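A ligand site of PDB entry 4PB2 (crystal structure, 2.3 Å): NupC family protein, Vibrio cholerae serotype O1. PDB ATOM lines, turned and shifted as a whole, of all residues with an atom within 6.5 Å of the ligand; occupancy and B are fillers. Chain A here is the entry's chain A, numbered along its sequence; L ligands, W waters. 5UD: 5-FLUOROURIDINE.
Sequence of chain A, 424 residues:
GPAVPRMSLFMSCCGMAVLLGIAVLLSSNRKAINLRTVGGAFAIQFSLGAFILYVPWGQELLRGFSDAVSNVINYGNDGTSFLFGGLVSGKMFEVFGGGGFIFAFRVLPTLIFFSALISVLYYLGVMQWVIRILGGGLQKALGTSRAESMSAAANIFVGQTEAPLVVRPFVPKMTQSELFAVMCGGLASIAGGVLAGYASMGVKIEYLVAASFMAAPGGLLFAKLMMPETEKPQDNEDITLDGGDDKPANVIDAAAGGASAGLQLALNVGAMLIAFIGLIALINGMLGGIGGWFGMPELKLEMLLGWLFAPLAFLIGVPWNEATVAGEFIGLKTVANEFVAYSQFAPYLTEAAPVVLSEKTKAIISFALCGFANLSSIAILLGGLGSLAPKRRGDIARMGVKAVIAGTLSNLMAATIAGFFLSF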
ATOM      1  N   LEU A 111      29.805 -38.976  23.123  1.00  0.00           N
ATOM      2  CA  LEU A 111      30.444 -37.860  23.829  1.00  0.00           C
ATOM      3  C   LEU A 111      31.849 -38.256  24.276  1.00  0.00           C
ATOM      4  O   LEU A 111      32.755 -37.429  24.318  1.00  0.00           O
ATOM      5  CB  LEU A 111      29.610 -37.425  25.033  1.00  0.00           C
ATOM      6  CG  LEU A 111      28.124 -37.121  24.848  1.00  0.00           C
ATOM      7  CD1 LEU A 111      27.536 -36.548  26.130  1.00  0.00           C
ATOM      8  CD2 LEU A 111      27.897 -36.181  23.686  1.00  0.00           C
ATOM      9  N   VAL A 158      34.749 -26.596  20.469  1.00  0.00           N
ATOM     10  CA  VAL A 158      34.714 -27.053  21.856  1.00  0.00           C
ATOM     11  C   VAL A 158      33.764 -26.230  22.727  1.00  0.00           C
ATOM     12  O   VAL A 158      33.229 -25.206  22.297  1.00  0.00           O
ATOM     13  CB  VAL A 158      36.119 -27.021  22.495  1.00  0.00           C
ATOM     14  CG1 VAL A 158      37.052 -27.979  21.770  1.00  0.00           C
ATOM     15  CG2 VAL A 158      36.674 -25.604  22.493  1.00  0.00           C
ATOM     16  N   GLY A 159      33.586 -26.675  23.969  1.00  0.00           N
ATOM     17  CA  GLY A 159      32.623 -26.080  24.884  1.00  0.00           C
ATOM     18  C   GLY A 159      33.062 -24.777  25.526  1.00  0.00           C
ATOM     19  O   GLY A 159      34.229 -24.386  25.462  1.00  0.00           O
ATOM     20  N   GLN A 160      32.100 -24.120  26.169  1.00  0.00           N
ATOM     21  CA  GLN A 160      32.277 -22.791  26.741  1.00  0.00           C
ATOM     22  C   GLN A 160      33.376 -22.691  27.797  1.00  0.00           C
ATOM     23  O   GLN A 160      33.927 -21.617  28.031  1.00  0.00           O
ATOM     24  CB  GLN A 160      30.964 -22.309  27.353  1.00  0.00           C
ATOM     25  CG  GLN A 160      30.365 -23.268  28.378  1.00  0.00           C
ATOM     26  CD  GLN A 160      29.006 -22.833  28.866  1.00  0.00           C
ATOM     27  OE1 GLN A 160      28.594 -21.685  28.650  1.00  0.00           O
ATOM     28  NE2 GLN A 160      28.286 -23.742  29.517  1.00  0.00           N
ATOM     29  N   THR A 161      33.699 -23.813  28.433  1.00  0.00           N
ATOM     30  CA  THR A 161      34.721 -23.813  29.466  1.00  0.00           C
ATOM     31  C   THR A 161      36.091 -24.203  28.911  1.00  0.00           C
ATOM     32  O   THR A 161      37.116 -23.892  29.496  1.00  0.00           O
ATOM     33  CB  THR A 161      34.352 -24.764  30.632  1.00  0.00           C
ATOM     34  OG1 THR A 161      33.972 -26.040  30.104  1.00  0.00           O
ATOM     35  CG2 THR A 161      33.210 -24.190  31.444  1.00  0.00           C
ATOM     36  N   GLU A 162      36.086 -24.883  27.767  1.00  0.00           N
ATOM     37  CA  GLU A 162      37.324 -25.361  27.158  1.00  0.00           C
ATOM     38  C   GLU A 162      37.898 -24.346  26.169  1.00  0.00           C
ATOM     39  O   GLU A 162      39.122 -24.225  26.024  1.00  0.00           O
ATOM     40  CB  GLU A 162      37.098 -26.700  26.457  1.00  0.00           C
ATOM     41  CG  GLU A 162      37.017 -27.899  27.390  1.00  0.00           C
ATOM     42  CD  GLU A 162      35.796 -27.868  28.281  1.00  0.00           C
ATOM     43  OE1 GLU A 162      34.698 -27.533  27.778  1.00  0.00           O
ATOM     44  OE2 GLU A 162      35.926 -28.182  29.480  1.00  0.00           O
ATOM     45  N   ILE A 190      27.893 -24.524  20.896  1.00  0.00           N
ATOM     46  CA  ILE A 190      27.847 -25.794  21.605  1.00  0.00           C
ATOM     47  C   ILE A 190      29.242 -26.404  21.645  1.00  0.00           C
ATOM     48  O   ILE A 190      30.234 -25.693  21.830  1.00  0.00           O
ATOM     49  CB  ILE A 190      26.845 -26.778  20.949  1.00  0.00           C
ATOM     50  CG1 ILE A 190      27.097 -26.903  19.454  1.00  0.00           C
ATOM     51  CG2 ILE A 190      25.418 -26.295  21.181  1.00  0.00           C
ATOM     52  CD1 ILE A 190      26.360 -28.073  18.807  1.00  0.00           C
ATOM     53  N   ALA A 191      29.330 -27.719  21.478  1.00  0.00           N
ATOM     54  CA  ALA A 191      30.618 -28.410  21.505  1.00  0.00           C
ATOM     55  C   ALA A 191      30.602 -29.588  20.542  1.00  0.00           C
ATOM     56  O   ALA A 191      29.549 -30.149  20.261  1.00  0.00           O
ATOM     57  CB  ALA A 191      30.950 -28.871  22.911  1.00  0.00           C
ATOM     58  N   GLY A 193      31.516 -32.569  20.942  1.00  0.00           N
ATOM     59  CA  GLY A 193      31.032 -33.781  21.565  1.00  0.00           C
ATOM     60  C   GLY A 193      29.523 -33.937  21.490  1.00  0.00           C
ATOM     61  O   GLY A 193      29.026 -34.951  21.005  1.00  0.00           O
ATOM     62  N   VAL A 194      28.795 -32.926  21.957  1.00  0.00           N
ATOM     63  CA  VAL A 194      27.333 -32.991  21.970  1.00  0.00           C
ATOM     64  C   VAL A 194      26.728 -32.800  20.582  1.00  0.00           C
ATOM     65  O   VAL A 194      25.599 -33.214  20.339  1.00  0.00           O
ATOM     66  CB  VAL A 194      26.735 -31.939  22.923  1.00  0.00           C
ATOM     67  CG1 VAL A 194      26.963 -32.356  24.372  1.00  0.00           C
ATOM     68  CG2 VAL A 194      27.315 -30.563  22.651  1.00  0.00           C
ATOM     69  N   TYR A 198      23.720 -34.869  19.280  1.00  0.00           N
ATOM     70  CA  TYR A 198      22.496 -34.360  18.683  1.00  0.00           C
ATOM     71  C   TYR A 198      22.288 -34.933  17.286  1.00  0.00           C
ATOM     72  O   TYR A 198      21.158 -35.231  16.881  1.00  0.00           O
ATOM     73  CB  TYR A 198      22.520 -32.832  18.637  1.00  0.00           C
ATOM     74  CG  TYR A 198      22.645 -32.181  19.991  1.00  0.00           C
ATOM     75  CD1 TYR A 198      22.085 -32.769  21.119  1.00  0.00           C
ATOM     76  CD2 TYR A 198      23.328 -30.975  20.147  1.00  0.00           C
ATOM     77  CE1 TYR A 198      22.201 -32.181  22.368  1.00  0.00           C
ATOM     78  CE2 TYR A 198      23.444 -30.387  21.395  1.00  0.00           C
ATOM     79  CZ  TYR A 198      22.882 -30.984  22.496  1.00  0.00           C
ATOM     80  OH  TYR A 198      22.997 -30.401  23.731  1.00  0.00           O
ATOM     81  N   LEU A 265      31.379 -36.076  31.318  1.00  0.00           N
ATOM     82  CA  LEU A 265      30.348 -35.323  30.612  1.00  0.00           C
ATOM     83  C   LEU A 265      29.140 -36.218  30.333  1.00  0.00           C
ATOM     84  O   LEU A 265      28.003 -35.825  30.563  1.00  0.00           O
ATOM     85  CB  LEU A 265      30.903 -34.747  29.310  1.00  0.00           C
ATOM     86  CG  LEU A 265      29.896 -34.056  28.400  1.00  0.00           C
ATOM     87  CD1 LEU A 265      29.273 -32.863  29.108  1.00  0.00           C
ATOM     88  CD2 LEU A 265      30.564 -33.626  27.094  1.00  0.00           C
ATOM     89  N   VAL A 269      25.391 -35.576  31.738  1.00  0.00           N
ATOM     90  CA  VAL A 269      24.289 -35.363  30.805  1.00  0.00           C
ATOM     91  C   VAL A 269      23.176 -36.384  31.044  1.00  0.00           C
ATOM     92  O   VAL A 269      22.005 -36.031  31.088  1.00  0.00           O
ATOM     93  CB  VAL A 269      24.759 -35.427  29.339  1.00  0.00           C
ATOM     94  CG1 VAL A 269      23.571 -35.467  28.387  1.00  0.00           C
ATOM     95  CG2 VAL A 269      25.672 -34.250  29.017  1.00  0.00           C
ATOM     96  N   MET A 272      21.346 -35.684  34.271  1.00  0.00           N
ATOM     97  CA  MET A 272      20.562 -34.471  34.083  1.00  0.00           C
ATOM     98  C   MET A 272      19.269 -34.777  33.325  1.00  0.00           C
ATOM     99  O   MET A 272      18.203 -34.277  33.673  1.00  0.00           O
ATOM    100  CB  MET A 272      21.382 -33.407  33.341  1.00  0.00           C
ATOM    101  CG  MET A 272      20.618 -32.124  33.003  1.00  0.00           C
ATOM    102  SD  MET A 272      19.742 -32.190  31.420  1.00  0.00           S
ATOM    103  CE  MET A 272      21.112 -32.377  30.281  1.00  0.00           C
ATOM    104  N   ALA A 336      15.609 -24.329  30.382  1.00  0.00           N
ATOM    105  CA  ALA A 336      16.381 -25.453  30.884  1.00  0.00           C
ATOM    106  C   ALA A 336      17.747 -25.532  30.201  1.00  0.00           C
ATOM    107  O   ALA A 336      18.704 -24.902  30.644  1.00  0.00           O
ATOM    108  CB  ALA A 336      15.609 -26.761  30.684  1.00  0.00           C
ATOM    109  N   ASN A 337      17.829 -26.319  29.132  1.00  0.00           N
ATOM    110  CA  ASN A 337      19.008 -26.361  28.284  1.00  0.00           C
ATOM    111  C   ASN A 337      18.689 -26.977  26.928  1.00  0.00           C
ATOM    112  O   ASN A 337      17.620 -27.554  26.741  1.00  0.00           O
ATOM    113  CB  ASN A 337      20.154 -27.131  28.959  1.00  0.00           C
ATOM    114  CG  ASN A 337      19.789 -28.571  29.263  1.00  0.00           C
ATOM    115  OD1 ASN A 337      19.742 -29.419  28.375  1.00  0.00           O
ATOM    116  ND2 ASN A 337      19.546 -28.861  30.540  1.00  0.00           N
ATOM    117  N   GLU A 338      19.621 -26.866  25.991  1.00  0.00           N
ATOM    118  CA  GLU A 338      19.371 -27.280  24.620  1.00  0.00           C
ATOM    119  C   GLU A 338      19.298 -28.794  24.472  1.00  0.00           C
ATOM    120  O   GLU A 338      18.643 -29.297  23.551  1.00  0.00           O
ATOM    121  CB  GLU A 338      20.456 -26.699  23.691  1.00  0.00           C
ATOM    122  CG  GLU A 338      21.754 -27.508  23.599  1.00  0.00           C
ATOM    123  CD  GLU A 338      22.556 -27.503  24.894  1.00  0.00           C
ATOM    124  OE1 GLU A 338      22.268 -26.672  25.789  1.00  0.00           O
ATOM    125  OE2 GLU A 338      23.477 -28.334  25.021  1.00  0.00           O
ATOM    126  N   PHE A 339      19.935 -29.521  25.375  1.00  0.00           N
ATOM    127  CA  PHE A 339      19.922 -30.978  25.302  1.00  0.00           C
ATOM    128  C   PHE A 339      18.522 -31.529  25.555  1.00  0.00           C
ATOM    129  O   PHE A 339      18.038 -32.376  24.808  1.00  0.00           O
ATOM    130  CB  PHE A 339      20.896 -31.590  26.308  1.00  0.00           C
ATOM    131  CG  PHE A 339      21.669 -32.756  25.769  1.00  0.00           C
ATOM    132  CD1 PHE A 339      23.049 -32.734  25.707  1.00  0.00           C
ATOM    133  CD2 PHE A 339      21.001 -33.885  25.306  1.00  0.00           C
ATOM    134  CE1 PHE A 339      23.748 -33.804  25.209  1.00  0.00           C
ATOM    135  CE2 PHE A 339      21.706 -34.952  24.799  1.00  0.00           C
ATOM    136  CZ  PHE A 339      23.080 -34.919  24.749  1.00  0.00           C
ATOM    137  N   VAL A 340      17.870 -31.036  26.598  1.00  0.00           N
ATOM    138  CA  VAL A 340      16.512 -31.440  26.913  1.00  0.00           C
ATOM    139  C   VAL A 340      15.559 -31.027  25.799  1.00  0.00           C
ATOM    140  O   VAL A 340      14.651 -31.783  25.438  1.00  0.00           O
ATOM    141  CB  VAL A 340      16.030 -30.831  28.245  1.00  0.00           C
ATOM    142  CG1 VAL A 340      14.654 -31.356  28.615  1.00  0.00           C
ATOM    143  CG2 VAL A 340      17.022 -31.131  29.352  1.00  0.00           C
ATOM    144  N   GLY A 371      22.738 -23.971  20.915  1.00  0.00           N
ATOM    145  CA  GLY A 371      23.515 -23.075  21.758  1.00  0.00           C
ATOM    146  C   GLY A 371      23.406 -23.439  23.230  1.00  0.00           C
ATOM    147  O   GLY A 371      22.401 -23.978  23.667  1.00  0.00           O
ATOM    148  N   PHE A 372      24.455 -23.128  23.985  1.00  0.00           N
ATOM    149  CA  PHE A 372      24.482 -23.384  25.423  1.00  0.00           C
ATOM    150  C   PHE A 372      23.843 -22.238  26.207  1.00  0.00           C
ATOM    151  O   PHE A 372      23.965 -22.175  27.435  1.00  0.00           O
ATOM    152  CB  PHE A 372      25.914 -23.609  25.919  1.00  0.00           C
ATOM    153  CG  PHE A 372      26.502 -24.937  25.515  1.00  0.00           C
ATOM    154  CD1 PHE A 372      25.726 -25.894  24.885  1.00  0.00           C
ATOM    155  CD2 PHE A 372      27.826 -25.233  25.794  1.00  0.00           C
ATOM    156  CE1 PHE A 372      26.270 -27.116  24.516  1.00  0.00           C
ATOM    157  CE2 PHE A 372      28.377 -26.458  25.441  1.00  0.00           C
ATOM    158  CZ  PHE A 372      27.593 -27.399  24.798  1.00  0.00           C
ATOM    159  N   ALA A 373      23.185 -21.330  25.492  1.00  0.00           N
ATOM    160  CA  ALA A 373      22.580 -20.159  26.110  1.00  0.00           C
ATOM    161  C   ALA A 373      21.412 -20.522  27.019  1.00  0.00           C
ATOM    162  O   ALA A 373      20.289 -20.706  26.563  1.00  0.00           O
ATOM    163  CB  ALA A 373      22.125 -19.172  25.048  1.00  0.00           C
ATOM    164  N   ASN A 374      21.699 -20.634  28.317  1.00  0.00           N
ATOM    165  CA  ASN A 374      20.678 -20.798  29.342  1.00  0.00           C
ATOM    166  C   ASN A 374      21.225 -20.342  30.677  1.00  0.00           C
ATOM    167  O   ASN A 374      22.436 -20.150  30.830  1.00  0.00           O
ATOM    168  CB  ASN A 374      20.187 -22.248  29.410  1.00  0.00           C
ATOM    169  CG  ASN A 374      21.289 -23.220  29.780  1.00  0.00           C
ATOM    170  OD1 ASN A 374      21.622 -23.381  30.950  1.00  0.00           O
ATOM    171  ND2 ASN A 374      21.850 -23.886  28.782  1.00  0.00           N
ATOM    172  N   SER A 376      21.528 -21.851  33.552  1.00  0.00           N
ATOM    173  CA  SER A 376      22.385 -22.811  34.244  1.00  0.00           C
ATOM    174  C   SER A 376      23.826 -22.776  33.743  1.00  0.00           C
ATOM    175  O   SER A 376      24.744 -23.165  34.459  1.00  0.00           O
ATOM    176  CB  SER A 376      21.831 -24.224  34.103  1.00  0.00           C
ATOM    177  OG  SER A 376      20.599 -24.352  34.792  1.00  0.00           O
ATOM    178  N   SER A 377      24.021 -22.297  32.520  1.00  0.00           N
ATOM    179  CA  SER A 377      25.374 -22.176  31.975  1.00  0.00           C
ATOM    180  C   SER A 377      26.171 -21.083  32.688  1.00  0.00           C
ATOM    181  O   SER A 377      27.407 -21.080  32.617  1.00  0.00           O
ATOM    182  CB  SER A 377      25.324 -21.900  30.480  1.00  0.00           C
ATOM    183  OG  SER A 377      24.976 -23.071  29.747  1.00  0.00           O
ATOM    184  N   ILE A 378      25.485 -20.158  33.351  1.00  0.00           N
ATOM    185  CA  ILE A 378      26.168 -19.121  34.124  1.00  0.00           C
ATOM    186  C   ILE A 378      27.012 -19.762  35.235  1.00  0.00           C
ATOM    187  O   ILE A 378      28.181 -19.416  35.400  1.00  0.00           O
ATOM    188  CB  ILE A 378      25.185 -18.112  34.746  1.00  0.00           C
ATOM    189  CG1 ILE A 378      24.336 -17.437  33.677  1.00  0.00           C
ATOM    190  CG2 ILE A 378      25.950 -17.063  35.548  1.00  0.00           C
ATOM    191  CD1 ILE A 378      23.287 -16.489  34.232  1.00  0.00           C
ATOM    192  N   ILE A 380      28.119 -22.717  35.267  1.00  0.00           N
ATOM    193  CA  ILE A 380      29.181 -23.447  34.583  1.00  0.00           C
ATOM    194  C   ILE A 380      30.345 -22.513  34.258  1.00  0.00           C
ATOM    195  O   ILE A 380      31.494 -22.846  34.506  1.00  0.00           O
ATOM    196  CB  ILE A 380      28.665 -24.098  33.278  1.00  0.00           C
ATOM    197  CG1 ILE A 380      27.512 -25.056  33.580  1.00  0.00           C
ATOM    198  CG2 ILE A 380      29.789 -24.834  32.571  1.00  0.00           C
ATOM    199  CD1 ILE A 380      27.890 -26.207  34.482  1.00  0.00           C
HETATM  200  F5  5UD L   1      28.626 -30.559  26.281  1.00  0.00           F
HETATM  201  C5  5UD L   1      28.709 -29.567  27.143  1.00  0.00           C
HETATM  202  C4  5UD L   1      29.961 -28.908  27.354  1.00  0.00           C
HETATM  203  O4  5UD L   1      30.958 -29.262  26.725  1.00  0.00           O
HETATM  204  N3  5UD L   1      30.038 -27.868  28.261  1.00  0.00           N
HETATM  205  C2  5UD L   1      28.910 -27.490  28.949  1.00  0.00           C
HETATM  206  O2  5UD L   1      28.971 -26.573  29.754  1.00  0.00           O
HETATM  207  C6  5UD L   1      27.621 -29.167  27.837  1.00  0.00           C
HETATM  208  N1  5UD L   1      27.727 -28.131  28.736  1.00  0.00           N
HETATM  209  C1' 5UD L   1      26.514 -27.699  29.493  1.00  0.00           C
HETATM  210  C2' 5UD L   1      25.856 -26.462  28.897  1.00  0.00           C
HETATM  211  O2' 5UD L   1      25.386 -25.626  29.933  1.00  0.00           O
HETATM  212  C3' 5UD L   1      24.677 -27.036  28.128  1.00  0.00           C
HETATM  213  O3' 5UD L   1      23.621 -26.088  28.067  1.00  0.00           O
HETATM  214  C4' 5UD L   1      24.284 -28.208  29.009  1.00  0.00           C
HETATM  215  O4' 5UD L   1      25.538 -28.727  29.526  1.00  0.00           O
HETATM  216  C5' 5UD L   1      23.610 -29.282  28.173  1.00  0.00           C
HETATM  217  O5' 5UD L   1      24.282 -29.690  26.983  1.00  0.00           O
HETATM  218  O   HOH W   1      33.769 -29.310  25.759  1.00  0.00           O
HETATM  219  O   HOH W   2      22.903 -25.624  31.328  1.00  0.00           O
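Merely in contact with the ligand: Ala 191 (3.8 Å), Val 194 (3.1 Å), Tyr 198 (3.6 Å), Leu 265 (3.7 Å), Asn 337 (3.7 Å), Phe 339 (3.5 Å), Phe 372 (3.4 Å) and Ile 380 (3.4 Å). 12 residues have an atom within 4 Å of the ligand: Gln 160, Ala 191, Val 194, Tyr 198, Leu 265, Asn 337, Glu 338, Phe 339, Phe 372, Asn 374, Ser 377 and Ile 380.
Water W2 lies within hydrogen-bond range of OD1 of Asn 374 (2.6 Å) and O2' of the ligand (2.8 Å). Water W1 lies within hydrogen-bond range of OE1 of Glu 162 (2.8 Å), O4 of the ligand (3.0 Å) and N of Gly 159 (3.2 Å).
OE2 of Glu 338 is in hydrogen-bond range of OH of Tyr 198 (2.5 Å). The backbone NH (N) of Ser 377 lies within hydrogen-bond range of the side-chain amide oxygen (OD1) of Asn 374 (3.1 Å). The side-chain hydroxyl of Ser 377 lies within hydrogen-bond range of the side-chain amide nitrogen of Gln 160 (3.4 Å). OG of Ser 377 lies within hydrogen-bond range of O of Phe 372. O of Phe 372 is in hydrogen-bond range of ND2 of Asn 374, 3.0 Å away. OD1 of Asn 374 is in hydrogen-bond range of N of Ser 376 (3.0 Å). The side-chain sulfur of Met 272 is in hydrogen-bond range of the side-chain amide nitrogen of Asn 337, at 3.4 Å. N of Val 340 lies within hydrogen-bond range of OD1 of Asn 337 (3.0 Å).
An oxygen (O5') of the ligand lies within hydrogen-bond range of the side-chain carboxylate (OE2) of Glu 338. OG of Ser 377 lies within hydrogen-bond range of O2' of the ligand, 2.6 Å away. The side-chain amide nitrogen (ND2) of Asn 374 lies within hydrogen-bond range of an oxygen (O3') of the ligand (2.9 Å). O2 of the ligand sits at hydrogen-bond distance from NE2 of Gln 160 (2.9 Å).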
